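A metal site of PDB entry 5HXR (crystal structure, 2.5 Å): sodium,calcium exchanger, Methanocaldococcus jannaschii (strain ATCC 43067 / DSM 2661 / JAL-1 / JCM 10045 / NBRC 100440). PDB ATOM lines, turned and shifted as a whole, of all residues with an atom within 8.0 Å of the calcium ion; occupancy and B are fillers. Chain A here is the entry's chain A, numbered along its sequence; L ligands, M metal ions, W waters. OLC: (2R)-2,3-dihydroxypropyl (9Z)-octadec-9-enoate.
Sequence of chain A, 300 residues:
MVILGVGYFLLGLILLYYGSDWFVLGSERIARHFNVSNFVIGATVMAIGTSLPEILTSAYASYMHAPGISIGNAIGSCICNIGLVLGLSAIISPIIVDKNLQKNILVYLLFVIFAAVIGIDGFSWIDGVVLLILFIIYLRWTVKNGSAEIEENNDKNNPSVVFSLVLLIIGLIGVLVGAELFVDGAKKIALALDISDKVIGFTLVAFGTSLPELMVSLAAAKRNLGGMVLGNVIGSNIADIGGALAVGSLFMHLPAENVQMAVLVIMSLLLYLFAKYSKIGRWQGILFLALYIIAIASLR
OG of Ser 124 lies within hydrogen-bond range of N of Asp 127, 3.4 Å away.
A ring nitrogen (NE2) of His 253 sits at hydrogen-bond distance from the backbone carbonyl oxygen of Asp 121, 3.3 Å away.
Of the 17 residues printed, 4 come within 4 Å of the calcium ion.
O of Ile 118 binds the calcium ion (2.4 Å).
The calcium ion is bound by an oxygen (O23) of the ligand.
O of Gly 122 binds the calcium ion (2.4 Å).
OD2 of Asp 127 is bound to the calcium ion, 2.5 Å away.
OD1 of Asp 121 binds the calcium ion (2.5 Å).
The calcium ion is bound by water W1.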
ATOM      1  N   ALA A 115      17.552 -15.858 -17.955  1.00  0.00           N
ATOM      2  CA  ALA A 115      17.927 -15.330 -16.652  1.00  0.00           C
ATOM      3  C   ALA A 115      18.937 -16.242 -15.963  1.00  0.00           C
ATOM      4  O   ALA A 115      19.916 -15.781 -15.367  1.00  0.00           O
ATOM      5  CB  ALA A 115      16.697 -15.150 -15.778  1.00  0.00           C
ATOM      6  N   ALA A 116      18.687 -17.554 -16.047  1.00  0.00           N
ATOM      7  CA  ALA A 116      19.533 -18.550 -15.405  1.00  0.00           C
ATOM      8  C   ALA A 116      20.969 -18.520 -15.928  1.00  0.00           C
ATOM      9  O   ALA A 116      21.923 -18.635 -15.162  1.00  0.00           O
ATOM     10  CB  ALA A 116      18.934 -19.933 -15.586  1.00  0.00           C
ATOM     11  N   VAL A 117      21.112 -18.354 -17.245  1.00  0.00           N
ATOM     12  CA  VAL A 117      22.420 -18.398 -17.877  1.00  0.00           C
ATOM     13  C   VAL A 117      23.249 -17.154 -17.549  1.00  0.00           C
ATOM     14  O   VAL A 117      24.434 -17.261 -17.233  1.00  0.00           O
ATOM     15  CB  VAL A 117      22.305 -18.538 -19.411  1.00  0.00           C
ATOM     16  CG1 VAL A 117      23.673 -18.512 -20.057  1.00  0.00           C
ATOM     17  CG2 VAL A 117      21.584 -19.822 -19.766  1.00  0.00           C
ATOM     18  N   ILE A 118      22.635 -15.982 -17.615  1.00  0.00           N
ATOM     19  CA  ILE A 118      23.362 -14.743 -17.339  1.00  0.00           C
ATOM     20  C   ILE A 118      23.599 -14.554 -15.845  1.00  0.00           C
ATOM     21  O   ILE A 118      24.307 -13.639 -15.435  1.00  0.00           O
ATOM     22  CB  ILE A 118      22.623 -13.501 -17.881  1.00  0.00           C
ATOM     23  CG1 ILE A 118      21.393 -13.174 -17.015  1.00  0.00           C
ATOM     24  CG2 ILE A 118      22.231 -13.702 -19.343  1.00  0.00           C
ATOM     25  CD1 ILE A 118      20.744 -11.861 -17.354  1.00  0.00           C
ATOM     26  N   GLY A 119      23.007 -15.419 -15.032  1.00  0.00           N
ATOM     27  CA  GLY A 119      23.159 -15.351 -13.589  1.00  0.00           C
ATOM     28  C   GLY A 119      24.180 -16.329 -13.051  1.00  0.00           C
ATOM     29  O   GLY A 119      24.443 -16.361 -11.852  1.00  0.00           O
ATOM     30  N   ILE A 120      24.765 -17.122 -13.951  1.00  0.00           N
ATOM     31  CA  ILE A 120      25.753 -18.121 -13.580  1.00  0.00           C
ATOM     32  C   ILE A 120      26.939 -17.486 -12.845  1.00  0.00           C
ATOM     33  O   ILE A 120      27.457 -18.035 -11.878  1.00  0.00           O
ATOM     34  CB  ILE A 120      26.264 -18.885 -14.823  1.00  0.00           C
ATOM     35  CG1 ILE A 120      25.134 -19.741 -15.405  1.00  0.00           C
ATOM     36  CG2 ILE A 120      27.463 -19.760 -14.479  1.00  0.00           C
ATOM     37  CD1 ILE A 120      25.516 -20.494 -16.667  1.00  0.00           C
ATOM     38  N   ASP A 121      27.346 -16.306 -13.305  1.00  0.00           N
ATOM     39  CA  ASP A 121      28.403 -15.551 -12.631  1.00  0.00           C
ATOM     40  C   ASP A 121      27.824 -14.416 -11.798  1.00  0.00           C
ATOM     41  O   ASP A 121      28.499 -13.420 -11.535  1.00  0.00           O
ATOM     42  CB  ASP A 121      29.395 -14.998 -13.667  1.00  0.00           C
ATOM     43  CG  ASP A 121      28.732 -14.083 -14.676  1.00  0.00           C
ATOM     44  OD1 ASP A 121      27.503 -14.161 -14.840  1.00  0.00           O
ATOM     45  OD2 ASP A 121      29.445 -13.269 -15.301  1.00  0.00           O
ATOM     46  N   GLY A 122      26.576 -14.579 -11.371  1.00  0.00           N
ATOM     47  CA  GLY A 122      25.888 -13.569 -10.588  1.00  0.00           C
ATOM     48  C   GLY A 122      25.171 -12.565 -11.469  1.00  0.00           C
ATOM     49  O   GLY A 122      25.259 -12.628 -12.689  1.00  0.00           O
ATOM     50  N   PHE A 123      24.452 -11.638 -10.839  1.00  0.00           N
ATOM     51  CA  PHE A 123      23.686 -10.642 -11.564  1.00  0.00           C
ATOM     52  C   PHE A 123      24.247  -9.233 -11.359  1.00  0.00           C
ATOM     53  O   PHE A 123      24.174  -8.689 -10.260  1.00  0.00           O
ATOM     54  CB  PHE A 123      22.214 -10.665 -11.143  1.00  0.00           C
ATOM     55  CG  PHE A 123      21.488 -11.907 -11.571  1.00  0.00           C
ATOM     56  CD1 PHE A 123      20.946 -12.006 -12.842  1.00  0.00           C
ATOM     57  CD2 PHE A 123      21.341 -12.975 -10.693  1.00  0.00           C
ATOM     58  CE1 PHE A 123      20.274 -13.141 -13.241  1.00  0.00           C
ATOM     59  CE2 PHE A 123      20.667 -14.116 -11.085  1.00  0.00           C
ATOM     60  CZ  PHE A 123      20.132 -14.192 -12.360  1.00  0.00           C
ATOM     61  N   SER A 124      24.808  -8.668 -12.432  1.00  0.00           N
ATOM     62  CA  SER A 124      25.299  -7.301 -12.384  1.00  0.00           C
ATOM     63  C   SER A 124      24.157  -6.328 -12.678  1.00  0.00           C
ATOM     64  O   SER A 124      23.051  -6.747 -13.046  1.00  0.00           O
ATOM     65  CB  SER A 124      26.435  -7.094 -13.387  1.00  0.00           C
ATOM     66  OG  SER A 124      25.956  -7.117 -14.722  1.00  0.00           O
ATOM     67  N   TRP A 125      24.424  -5.039 -12.512  1.00  0.00           N
ATOM     68  CA  TRP A 125      23.412  -4.015 -12.747  1.00  0.00           C
ATOM     69  C   TRP A 125      23.027  -3.960 -14.228  1.00  0.00           C
ATOM     70  O   TRP A 125      21.929  -3.529 -14.572  1.00  0.00           O
ATOM     71  CB  TRP A 125      23.913  -2.652 -12.273  1.00  0.00           C
ATOM     72  CG  TRP A 125      25.142  -2.175 -12.980  1.00  0.00           C
ATOM     73  CD1 TRP A 125      26.433  -2.438 -12.643  1.00  0.00           C
ATOM     74  CD2 TRP A 125      25.193  -1.363 -14.158  1.00  0.00           C
ATOM     75  NE1 TRP A 125      27.297  -1.838 -13.529  1.00  0.00           N
ATOM     76  CE2 TRP A 125      26.554  -1.171 -14.468  1.00  0.00           C
ATOM     77  CE3 TRP A 125      24.228  -0.763 -14.969  1.00  0.00           C
ATOM     78  CZ2 TRP A 125      26.970  -0.407 -15.565  1.00  0.00           C
ATOM     79  CZ3 TRP A 125      24.639  -0.012 -16.052  1.00  0.00           C
ATOM     80  CH2 TRP A 125      25.998   0.154 -16.344  1.00  0.00           C
ATOM     81  N   ILE A 126      23.933  -4.398 -15.093  1.00  0.00           N
ATOM     82  CA  ILE A 126      23.648  -4.465 -16.524  1.00  0.00           C
ATOM     83  C   ILE A 126      22.699  -5.631 -16.810  1.00  0.00           C
ATOM     84  O   ILE A 126      21.823  -5.526 -17.669  1.00  0.00           O
ATOM     85  CB  ILE A 126      24.931  -4.612 -17.364  1.00  0.00           C
ATOM     86  CG1 ILE A 126      25.871  -3.429 -17.094  1.00  0.00           C
ATOM     87  CG2 ILE A 126      24.603  -4.684 -18.842  1.00  0.00           C
ATOM     88  CD1 ILE A 126      27.090  -3.412 -18.004  1.00  0.00           C
ATOM     89  N   ASP A 127      22.886  -6.729 -16.079  1.00  0.00           N
ATOM     90  CA  ASP A 127      21.960  -7.853 -16.155  1.00  0.00           C
ATOM     91  C   ASP A 127      20.563  -7.400 -15.771  1.00  0.00           C
ATOM     92  O   ASP A 127      19.567  -7.820 -16.363  1.00  0.00           O
ATOM     93  CB  ASP A 127      22.409  -9.004 -15.260  1.00  0.00           C
ATOM     94  CG  ASP A 127      23.677  -9.678 -15.744  1.00  0.00           C
ATOM     95  OD1 ASP A 127      23.985  -9.553 -16.947  1.00  0.00           O
ATOM     96  OD2 ASP A 127      24.352 -10.326 -14.922  1.00  0.00           O
ATOM     97  N   GLY A 128      20.493  -6.527 -14.765  1.00  0.00           N
ATOM     98  CA  GLY A 128      19.231  -6.021 -14.274  1.00  0.00           C
ATOM     99  C   GLY A 128      18.501  -5.158 -15.284  1.00  0.00           C
ATOM    100  O   GLY A 128      17.295  -5.285 -15.455  1.00  0.00           O
ATOM    101  N   HIS A 253      25.952  -6.091  -6.899  1.00  0.00           N
ATOM    102  CA  HIS A 253      26.074  -7.376  -7.563  1.00  0.00           C
ATOM    103  C   HIS A 253      25.433  -8.491  -6.727  1.00  0.00           C
ATOM    104  O   HIS A 253      25.831  -8.720  -5.586  1.00  0.00           O
ATOM    105  CB  HIS A 253      27.535  -7.717  -7.842  1.00  0.00           C
ATOM    106  CG  HIS A 253      27.737  -9.018  -8.562  1.00  0.00           C
ATOM    107  ND1 HIS A 253      27.750  -9.115  -9.934  1.00  0.00           N
ATOM    108  CD2 HIS A 253      27.921 -10.277  -8.097  1.00  0.00           C
ATOM    109  CE1 HIS A 253      27.942 -10.369 -10.286  1.00  0.00           C
ATOM    110  NE2 HIS A 253      28.042 -11.098  -9.191  1.00  0.00           N
ATOM    111  N   LEU A 254      24.441  -9.159  -7.302  1.00  0.00           N
ATOM    112  CA  LEU A 254      23.802 -10.281  -6.635  1.00  0.00           C
ATOM    113  C   LEU A 254      24.605 -11.553  -6.895  1.00  0.00           C
ATOM    114  O   LEU A 254      24.786 -11.951  -8.050  1.00  0.00           O
ATOM    115  CB  LEU A 254      22.362 -10.461  -7.124  1.00  0.00           C
ATOM    116  CG  LEU A 254      21.481  -9.213  -7.171  1.00  0.00           C
ATOM    117  CD1 LEU A 254      20.086  -9.567  -7.688  1.00  0.00           C
ATOM    118  CD2 LEU A 254      21.389  -8.556  -5.800  1.00  0.00           C
ATOM    119  N   ALA A 256      25.669 -15.476  -7.286  1.00  0.00           N
ATOM    120  CA  ALA A 256      24.970 -16.508  -8.043  1.00  0.00           C
ATOM    121  C   ALA A 256      24.257 -17.508  -7.142  1.00  0.00           C
ATOM    122  O   ALA A 256      24.786 -17.940  -6.124  1.00  0.00           O
ATOM    123  CB  ALA A 256      25.940 -17.231  -8.959  1.00  0.00           C
HETATM  124  C24 OLC L   1      27.978 -11.625 -17.970  1.00  0.00           C
HETATM  125  C2  OLC L   1      25.197  -7.936 -20.378  1.00  0.00           C
HETATM  126  C21 OLC L   1      26.114 -11.430 -19.644  1.00  0.00           C
HETATM  127  C1  OLC L   1      25.325  -9.461 -20.441  1.00  0.00           C
HETATM  128  C22 OLC L   1      26.577 -12.118 -18.364  1.00  0.00           C
HETATM  129  O19 OLC L   1      24.763 -10.097 -21.325  1.00  0.00           O
HETATM  130  O25 OLC L   1      27.962 -10.215 -17.765  1.00  0.00           O
HETATM  131  O23 OLC L   1      25.657 -11.806 -17.312  1.00  0.00           O
HETATM  132  O20 OLC L   1      26.070 -10.014 -19.457  1.00  0.00           O
HETATM  133 CA    CA M   1      26.066 -12.131 -14.935  1.00  0.00          CA
HETATM  134  O   HOH W   1      27.461 -10.069 -14.193  1.00  0.00           O
